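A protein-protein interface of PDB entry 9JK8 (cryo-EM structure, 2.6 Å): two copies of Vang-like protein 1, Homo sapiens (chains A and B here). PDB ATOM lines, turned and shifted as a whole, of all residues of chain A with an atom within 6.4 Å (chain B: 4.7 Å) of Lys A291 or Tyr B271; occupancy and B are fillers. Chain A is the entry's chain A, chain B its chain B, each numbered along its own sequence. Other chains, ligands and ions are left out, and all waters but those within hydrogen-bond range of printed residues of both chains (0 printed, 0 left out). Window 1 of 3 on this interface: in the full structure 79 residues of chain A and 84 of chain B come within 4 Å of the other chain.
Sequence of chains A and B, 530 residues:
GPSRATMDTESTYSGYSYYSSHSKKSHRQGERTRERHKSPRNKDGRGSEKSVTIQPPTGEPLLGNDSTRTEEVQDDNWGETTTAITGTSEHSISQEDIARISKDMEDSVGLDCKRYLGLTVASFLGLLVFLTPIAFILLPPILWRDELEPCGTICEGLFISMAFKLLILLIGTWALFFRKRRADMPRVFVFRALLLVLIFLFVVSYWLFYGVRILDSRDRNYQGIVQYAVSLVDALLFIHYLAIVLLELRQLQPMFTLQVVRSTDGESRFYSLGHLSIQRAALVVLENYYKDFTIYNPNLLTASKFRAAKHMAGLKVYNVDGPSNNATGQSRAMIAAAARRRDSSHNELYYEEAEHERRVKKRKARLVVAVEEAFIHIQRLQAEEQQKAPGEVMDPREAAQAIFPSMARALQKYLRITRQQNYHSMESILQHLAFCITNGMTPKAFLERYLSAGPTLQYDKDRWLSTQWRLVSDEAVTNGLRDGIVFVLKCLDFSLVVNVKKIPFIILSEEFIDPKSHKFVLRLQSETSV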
ATOM      1  N   TYR A 271      15.576  22.857  40.215  1.00  0.00           N
ATOM      2  CA  TYR A 271      16.645  22.014  39.688  1.00  0.00           C
ATOM      3  C   TYR A 271      17.429  21.388  40.832  1.00  0.00           C
ATOM      4  O   TYR A 271      17.842  22.105  41.755  1.00  0.00           O
ATOM      5  CB  TYR A 271      17.589  22.832  38.798  1.00  0.00           C
ATOM      6  CG  TYR A 271      16.924  23.489  37.604  1.00  0.00           C
ATOM      7  CD1 TYR A 271      16.534  22.745  36.496  1.00  0.00           C
ATOM      8  CD2 TYR A 271      16.687  24.859  37.587  1.00  0.00           C
ATOM      9  CE1 TYR A 271      15.927  23.349  35.407  1.00  0.00           C
ATOM     10  CE2 TYR A 271      16.082  25.469  36.504  1.00  0.00           C
ATOM     11  CZ  TYR A 271      15.704  24.711  35.418  1.00  0.00           C
ATOM     12  OH  TYR A 271      15.102  25.318  34.338  1.00  0.00           O
ATOM     13  N   LEU A 286      22.069  28.735  34.270  1.00  0.00           N
ATOM     14  CA  LEU A 286      21.980  29.446  32.994  1.00  0.00           C
ATOM     15  C   LEU A 286      21.816  28.491  31.814  1.00  0.00           C
ATOM     16  O   LEU A 286      21.071  28.789  30.867  1.00  0.00           O
ATOM     17  CB  LEU A 286      23.207  30.334  32.798  1.00  0.00           C
ATOM     18  CG  LEU A 286      23.236  31.517  33.764  1.00  0.00           C
ATOM     19  CD1 LEU A 286      24.517  32.313  33.623  1.00  0.00           C
ATOM     20  CD2 LEU A 286      22.019  32.394  33.530  1.00  0.00           C
ATOM     21  N   GLU A 287      22.521  27.359  31.841  1.00  0.00           N
ATOM     22  CA  GLU A 287      22.291  26.317  30.846  1.00  0.00           C
ATOM     23  C   GLU A 287      20.813  25.945  30.806  1.00  0.00           C
ATOM     24  O   GLU A 287      20.170  25.968  29.743  1.00  0.00           O
ATOM     25  CB  GLU A 287      23.141  25.093  31.194  1.00  0.00           C
ATOM     26  CG  GLU A 287      24.641  25.311  31.059  1.00  0.00           C
ATOM     27  CD  GLU A 287      25.452  24.192  31.693  1.00  0.00           C
ATOM     28  OE1 GLU A 287      24.844  23.262  32.263  1.00  0.00           O
ATOM     29  OE2 GLU A 287      26.696  24.266  31.668  1.00  0.00           O
ATOM     30  N   ASN A 288      20.245  25.663  31.978  1.00  0.00           N
ATOM     31  CA  ASN A 288      18.834  25.330  32.082  1.00  0.00           C
ATOM     32  C   ASN A 288      17.923  26.522  31.814  1.00  0.00           C
ATOM     33  O   ASN A 288      16.755  26.320  31.479  1.00  0.00           O
ATOM     34  CB  ASN A 288      18.546  24.747  33.465  1.00  0.00           C
ATOM     35  CG  ASN A 288      19.207  23.398  33.673  1.00  0.00           C
ATOM     36  OD1 ASN A 288      19.213  22.554  32.778  1.00  0.00           O
ATOM     37  ND2 ASN A 288      19.776  23.192  34.855  1.00  0.00           N
ATOM     38  N   TYR A 289      18.418  27.753  31.962  1.00  0.00           N
ATOM     39  CA  TYR A 289      17.619  28.919  31.600  1.00  0.00           C
ATOM     40  C   TYR A 289      17.429  28.998  30.097  1.00  0.00           C
ATOM     41  O   TYR A 289      16.306  29.170  29.609  1.00  0.00           O
ATOM     42  CB  TYR A 289      18.273  30.207  32.101  1.00  0.00           C
ATOM     43  CG  TYR A 289      17.514  31.432  31.638  1.00  0.00           C
ATOM     44  CD1 TYR A 289      16.301  31.774  32.215  1.00  0.00           C
ATOM     45  CD2 TYR A 289      17.983  32.212  30.587  1.00  0.00           C
ATOM     46  CE1 TYR A 289      15.590  32.877  31.786  1.00  0.00           C
ATOM     47  CE2 TYR A 289      17.276  33.318  30.147  1.00  0.00           C
ATOM     48  CZ  TYR A 289      16.080  33.644  30.753  1.00  0.00           C
ATOM     49  OH  TYR A 289      15.367  34.740  30.325  1.00  0.00           O
ATOM     50  N   TYR A 290      18.523  28.889  29.346  1.00  0.00           N
ATOM     51  CA  TYR A 290      18.397  28.914  27.896  1.00  0.00           C
ATOM     52  C   TYR A 290      17.656  27.696  27.373  1.00  0.00           C
ATOM     53  O   TYR A 290      17.032  27.774  26.309  1.00  0.00           O
ATOM     54  CB  TYR A 290      19.768  29.027  27.231  1.00  0.00           C
ATOM     55  CG  TYR A 290      20.428  30.359  27.484  1.00  0.00           C
ATOM     56  CD1 TYR A 290      19.961  31.510  26.868  1.00  0.00           C
ATOM     57  CD2 TYR A 290      21.523  30.464  28.327  1.00  0.00           C
ATOM     58  CE1 TYR A 290      20.555  32.732  27.096  1.00  0.00           C
ATOM     59  CE2 TYR A 290      22.129  31.682  28.558  1.00  0.00           C
ATOM     60  CZ  TYR A 290      21.641  32.813  27.939  1.00  0.00           C
ATOM     61  OH  TYR A 290      22.240  34.029  28.164  1.00  0.00           O
ATOM     62  N   LYS A 291      17.692  26.580  28.102  1.00  0.00           N
ATOM     63  CA  LYS A 291      16.914  25.424  27.677  1.00  0.00           C
ATOM     64  C   LYS A 291      15.425  25.548  27.983  1.00  0.00           C
ATOM     65  O   LYS A 291      14.585  25.238  27.132  1.00  0.00           O
ATOM     66  CB  LYS A 291      17.392  24.178  28.379  1.00  0.00           C
ATOM     67  CG  LYS A 291      16.695  22.969  27.865  1.00  0.00           C
ATOM     68  CD  LYS A 291      17.194  21.863  28.660  1.00  0.00           C
ATOM     69  CE  LYS A 291      18.552  21.544  28.265  1.00  0.00           C
ATOM     70  NZ  LYS A 291      18.826  20.357  29.075  1.00  0.00           N
ATOM     71  N   ASP A 292      15.086  25.938  29.210  1.00  0.00           N
ATOM     72  CA  ASP A 292      13.790  25.643  29.808  1.00  0.00           C
ATOM     73  C   ASP A 292      12.879  26.855  29.909  1.00  0.00           C
ATOM     74  O   ASP A 292      11.705  26.776  29.532  1.00  0.00           O
ATOM     75  CB  ASP A 292      13.996  25.040  31.208  1.00  0.00           C
ATOM     76  CG  ASP A 292      14.691  23.689  31.170  1.00  0.00           C
ATOM     77  OD1 ASP A 292      14.361  22.873  30.284  1.00  0.00           O
ATOM     78  OD2 ASP A 292      15.565  23.443  32.029  1.00  0.00           O
ATOM     79  N   PHE A 293      13.381  27.972  30.424  1.00  0.00           N
ATOM     80  CA  PHE A 293      12.547  29.155  30.584  1.00  0.00           C
ATOM     81  C   PHE A 293      12.176  29.737  29.228  1.00  0.00           C
ATOM     82  O   PHE A 293      12.966  29.704  28.282  1.00  0.00           O
ATOM     83  CB  PHE A 293      13.273  30.212  31.416  1.00  0.00           C
ATOM     84  CG  PHE A 293      13.425  29.849  32.863  1.00  0.00           C
ATOM     85  CD1 PHE A 293      14.489  29.071  33.288  1.00  0.00           C
ATOM     86  CD2 PHE A 293      12.508  30.290  33.801  1.00  0.00           C
ATOM     87  CE1 PHE A 293      14.633  28.739  34.621  1.00  0.00           C
ATOM     88  CE2 PHE A 293      12.647  29.960  35.134  1.00  0.00           C
ATOM     89  CZ  PHE A 293      13.711  29.183  35.545  1.00  0.00           C
ATOM     90  N   PRO A 455      11.263  28.790  24.431  1.00  0.00           N
ATOM     91  CA  PRO A 455      12.474  29.158  25.178  1.00  0.00           C
ATOM     92  C   PRO A 455      13.458  29.978  24.360  1.00  0.00           C
ATOM     93  O   PRO A 455      13.229  30.258  23.178  1.00  0.00           O
ATOM     94  CB  PRO A 455      13.067  27.800  25.578  1.00  0.00           C
ATOM     95  CG  PRO A 455      12.522  26.845  24.591  1.00  0.00           C
ATOM     96  CD  PRO A 455      11.157  27.338  24.223  1.00  0.00           C
ATOM     97  N   THR A 456      14.572  30.354  24.991  1.00  0.00           N
ATOM     98  CA  THR A 456      15.473  31.345  24.411  1.00  0.00           C
ATOM     99  C   THR A 456      16.261  30.788  23.228  1.00  0.00           C
ATOM    100  O   THR A 456      16.665  31.552  22.344  1.00  0.00           O
ATOM    101  CB  THR A 456      16.423  31.866  25.491  1.00  0.00           C
ATOM    102  OG1 THR A 456      15.673  32.193  26.667  1.00  0.00           O
ATOM    103  CG2 THR A 456      17.148  33.114  25.015  1.00  0.00           C
ATOM    104  N   LEU A 457      16.485  29.476  23.184  1.00  0.00           N
ATOM    105  CA  LEU A 457      17.330  28.887  22.152  1.00  0.00           C
ATOM    106  C   LEU A 457      16.590  28.581  20.853  1.00  0.00           C
ATOM    107  O   LEU A 457      17.218  28.097  19.907  1.00  0.00           O
ATOM    108  CB  LEU A 457      18.001  27.615  22.678  1.00  0.00           C
ATOM    109  CG  LEU A 457      19.077  27.858  23.737  1.00  0.00           C
ATOM    110  CD1 LEU A 457      19.463  26.562  24.431  1.00  0.00           C
ATOM    111  CD2 LEU A 457      20.296  28.518  23.111  1.00  0.00           C
ATOM    112  N   PHE B 256      25.821  20.399  24.517  1.00  0.00           N
ATOM    113  CA  PHE B 256      24.929  20.787  23.435  1.00  0.00           C
ATOM    114  C   PHE B 256      23.488  20.764  23.925  1.00  0.00           C
ATOM    115  O   PHE B 256      23.159  20.138  24.934  1.00  0.00           O
ATOM    116  CB  PHE B 256      25.079  19.839  22.236  1.00  0.00           C
ATOM    117  CG  PHE B 256      26.442  19.855  21.611  1.00  0.00           C
ATOM    118  CD1 PHE B 256      26.823  20.884  20.766  1.00  0.00           C
ATOM    119  CD2 PHE B 256      27.341  18.833  21.865  1.00  0.00           C
ATOM    120  CE1 PHE B 256      28.081  20.894  20.192  1.00  0.00           C
ATOM    121  CE2 PHE B 256      28.597  18.838  21.292  1.00  0.00           C
ATOM    122  CZ  PHE B 256      28.967  19.869  20.455  1.00  0.00           C
ATOM    123  N   THR B 257      22.620  21.446  23.180  1.00  0.00           N
ATOM    124  CA  THR B 257      21.182  21.390  23.385  1.00  0.00           C
ATOM    125  C   THR B 257      20.534  20.851  22.120  1.00  0.00           C
ATOM    126  O   THR B 257      20.980  21.143  21.005  1.00  0.00           O
ATOM    127  CB  THR B 257      20.605  22.766  23.737  1.00  0.00           C
ATOM    128  OG1 THR B 257      21.210  23.240  24.944  1.00  0.00           O
ATOM    129  CG2 THR B 257      19.105  22.686  23.957  1.00  0.00           C
ATOM    130  N   LEU B 258      19.500  20.041  22.294  1.00  0.00           N
ATOM    131  CA  LEU B 258      18.816  19.383  21.190  1.00  0.00           C
ATOM    132  C   LEU B 258      17.351  19.771  21.269  1.00  0.00           C
ATOM    133  O   LEU B 258      16.678  19.459  22.261  1.00  0.00           O
ATOM    134  CB  LEU B 258      18.993  17.866  21.262  1.00  0.00           C
ATOM    135  CG  LEU B 258      20.315  17.323  20.715  1.00  0.00           C
ATOM    136  CD1 LEU B 258      21.462  17.558  21.689  1.00  0.00           C
ATOM    137  CD2 LEU B 258      20.186  15.847  20.385  1.00  0.00           C
ATOM    138  N   VAL B 260      13.920  18.873  19.946  1.00  0.00           N
ATOM    139  CA  VAL B 260      13.269  17.701  19.378  1.00  0.00           C
ATOM    140  C   VAL B 260      11.813  18.078  19.153  1.00  0.00           C
ATOM    141  O   VAL B 260      11.092  18.397  20.109  1.00  0.00           O
ATOM    142  CB  VAL B 260      13.395  16.483  20.303  1.00  0.00           C
ATOM    143  CG1 VAL B 260      12.720  15.267  19.688  1.00  0.00           C
ATOM    144  CG2 VAL B 260      14.856  16.204  20.627  1.00  0.00           C
ATOM    145  N   ARG B 269      10.487  19.667  22.724  1.00  0.00           N
ATOM    146  CA  ARG B 269      11.194  19.667  23.996  1.00  0.00           C
ATOM    147  C   ARG B 269      12.694  19.773  23.754  1.00  0.00           C
ATOM    148  O   ARG B 269      13.214  19.291  22.744  1.00  0.00           O
ATOM    149  CB  ARG B 269      10.865  18.408  24.829  1.00  0.00           C
ATOM    150  CG  ARG B 269       9.413  18.343  25.317  1.00  0.00           C
ATOM    151  CD  ARG B 269       9.142  17.101  26.162  1.00  0.00           C
ATOM    152  NE  ARG B 269       7.741  16.988  26.556  1.00  0.00           N
ATOM    153  CZ  ARG B 269       7.215  17.519  27.652  1.00  0.00           C
ATOM    154  NH1 ARG B 269       7.947  18.220  28.502  1.00  0.00           N
ATOM    155  NH2 ARG B 269       5.921  17.340  27.903  1.00  0.00           N
ATOM    156  N   PHE B 270      13.388  20.422  24.686  1.00  0.00           N
ATOM    157  CA  PHE B 270      14.833  20.579  24.628  1.00  0.00           C
ATOM    158  C   PHE B 270      15.526  19.624  25.593  1.00  0.00           C
ATOM    159  O   PHE B 270      14.980  19.253  26.632  1.00  0.00           O
ATOM    160  CB  PHE B 270      15.263  22.015  24.953  1.00  0.00           C
ATOM    161  CG  PHE B 270      14.873  23.029  23.916  1.00  0.00           C
ATOM    162  CD1 PHE B 270      13.550  23.249  23.582  1.00  0.00           C
ATOM    163  CD2 PHE B 270      15.852  23.772  23.279  1.00  0.00           C
ATOM    164  CE1 PHE B 270      13.214  24.186  22.625  1.00  0.00           C
ATOM    165  CE2 PHE B 270      15.525  24.711  22.327  1.00  0.00           C
ATOM    166  CZ  PHE B 270      14.204  24.921  22.000  1.00  0.00           C
ATOM    167  N   TYR B 271      16.748  19.229  25.229  1.00  0.00           N
ATOM    168  CA  TYR B 271      17.538  18.326  26.061  1.00  0.00           C
ATOM    169  C   TYR B 271      19.013  18.691  25.972  1.00  0.00           C
ATOM    170  O   TYR B 271      19.539  18.846  24.861  1.00  0.00           O
ATOM    171  CB  TYR B 271      17.336  16.871  25.624  1.00  0.00           C
ATOM    172  CG  TYR B 271      15.902  16.383  25.691  1.00  0.00           C
ATOM    173  CD1 TYR B 271      15.295  16.094  26.909  1.00  0.00           C
ATOM    174  CD2 TYR B 271      15.155  16.208  24.532  1.00  0.00           C
ATOM    175  CE1 TYR B 271      13.985  15.647  26.966  1.00  0.00           C
ATOM    176  CE2 TYR B 271      13.846  15.763  24.581  1.00  0.00           C
ATOM    177  CZ  TYR B 271      13.267  15.484  25.799  1.00  0.00           C
ATOM    178  OH  TYR B 271      11.965  15.040  25.849  1.00  0.00           O
ATOM    179  N   SER B 272      19.695  18.824  27.108  1.00  0.00           N
ATOM    180  CA  SER B 272      21.155  18.951  27.098  1.00  0.00           C
ATOM    181  C   SER B 272      21.786  17.589  26.974  1.00  0.00           C
ATOM    182  O   SER B 272      21.399  16.634  27.651  1.00  0.00           O
ATOM    183  CB  SER B 272      21.718  19.629  28.348  1.00  0.00           C
ATOM    184  OG  SER B 272      21.478  21.022  28.395  1.00  0.00           O
ATOM    185  N   LEU B 273      22.798  17.510  26.116  1.00  0.00           N
ATOM    186  CA  LEU B 273      23.610  16.321  25.988  1.00  0.00           C
ATOM    187  C   LEU B 273      25.069  16.742  25.998  1.00  0.00           C
ATOM    188  O   LEU B 273      25.389  17.921  25.816  1.00  0.00           O
ATOM    189  CB  LEU B 273      23.256  15.543  24.718  1.00  0.00           C
ATOM    190  CG  LEU B 273      21.832  14.998  24.813  1.00  0.00           C
ATOM    191  CD1 LEU B 273      21.320  14.471  23.485  1.00  0.00           C
ATOM    192  CD2 LEU B 273      21.773  13.938  25.890  1.00  0.00           C
ATOM    193  N   ASN B 288      14.029   9.761  25.918  1.00  0.00           N
ATOM    194  CA  ASN B 288      13.245  10.902  26.359  1.00  0.00           C
ATOM    195  C   ASN B 288      11.956  11.078  25.565  1.00  0.00           C
ATOM    196  O   ASN B 288      11.032  11.724  26.060  1.00  0.00           O
ATOM    197  CB  ASN B 288      14.095  12.169  26.272  1.00  0.00           C
ATOM    198  CG  ASN B 288      15.240  12.169  27.265  1.00  0.00           C
ATOM    199  OD1 ASN B 288      15.076  11.768  28.418  1.00  0.00           O
ATOM    200  ND2 ASN B 288      16.412  12.608  26.821  1.00  0.00           N
ATOM    201  N   ASP B 292       8.705  11.472  27.674  1.00  0.00           N
ATOM    202  CA  ASP B 292       8.275  12.854  27.839  1.00  0.00           C
ATOM    203  C   ASP B 292       7.192  13.271  26.858  1.00  0.00           C
ATOM    204  O   ASP B 292       6.187  13.864  27.264  1.00  0.00           O
ATOM    205  CB  ASP B 292       9.486  13.790  27.692  1.00  0.00           C
ATOM    206  CG  ASP B 292      10.512  13.600  28.797  1.00  0.00           C
ATOM    207  OD1 ASP B 292      10.107  13.436  29.967  1.00  0.00           O
ATOM    208  OD2 ASP B 292      11.724  13.620  28.493  1.00  0.00           O
ATOM    209  N   PHE B 293       7.375  12.994  25.570  1.00  0.00           N
ATOM    210  CA  PHE B 293       6.393  13.404  24.577  1.00  0.00           C
ATOM    211  C   PHE B 293       5.101  12.618  24.745  1.00  0.00           C
ATOM    212  O   PHE B 293       5.113  11.437  25.099  1.00  0.00           O
ATOM    213  CB  PHE B 293       6.941  13.196  23.165  1.00  0.00           C
ATOM    214  CG  PHE B 293       8.043  14.145  22.794  1.00  0.00           C
ATOM    215  CD1 PHE B 293       9.357  13.868  23.131  1.00  0.00           C
ATOM    216  CD2 PHE B 293       7.766  15.311  22.103  1.00  0.00           C
ATOM    217  CE1 PHE B 293      10.373  14.737  22.788  1.00  0.00           C
ATOM    218  CE2 PHE B 293       8.777  16.185  21.758  1.00  0.00           C
ATOM    219  CZ  PHE B 293      10.082  15.898  22.101  1.00  0.00           C
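Hydrophobic or aromatic side chains of chain A within 4 Å of the printed part of chain B: Pro A455 and Leu A457.
Of the 12 printed residues of chain B, 4 touch a printed residue of chain A.
Printed residues of chain B that touch a printed residue of chain A: Thr B257, Phe B270, Tyr B271 and Ser B272.
Hydrophobic or aromatic side chains of chain B that line the printed part of chain A: Phe B270.
Lys A291 touches three residues of chain B.
Of chain A, only Lys A291 comes within 4 Å of Tyr B271.
Of the printed residues of chain A, Thr B257 touches Leu A457 (3.8 Å).
Of the printed residues of chain B, Leu A457 touches Thr B257 (3.8 Å) and Phe B270 (3.8 Å).
Of the printed residues of chain B, Pro A455 touches Phe B270 (3.4 Å).
Of the printed residues of chain A, Phe B270 touches Lys A291 (3.4 Å), Pro A455 (3.4 Å) and Leu A457 (3.8 Å).
Arg B269 touches none of the printed residues of chain A.
The nearest printed residue of chain A that does not touch Tyr B271 is Asp A292 (6.7 Å).
Positions printed for both chains: 271, 288, 292 and 293.
Among the printed residues, pairs that only touch across the chains: Lys A291 with Phe B270 (3.4 Å), Lys A291 with Tyr B271 (3.5 Å), Pro A455 with Phe B270 (3.4 Å), Leu A457 with Thr B257 (3.8 Å) and Leu A457 with Phe B270 (3.8 Å).
NZ of Lys A291 sits at hydrogen-bond distance from OG of Ser B272, at 2.8 Å.
The side-chain carboxylate (OD2) of Asp B292 is in hydrogen-bond range of the side-chain hydroxyl (OH) of Tyr B271, 3.0 Å away.
The backbone NH (N) of Leu B258 is in hydrogen-bond range of the backbone carbonyl oxygen (O) of Tyr B271.
The side-chain hydroxyl of Tyr B271 is in hydrogen-bond range of the backbone carbonyl oxygen of Asn B288 (3.5 Å).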
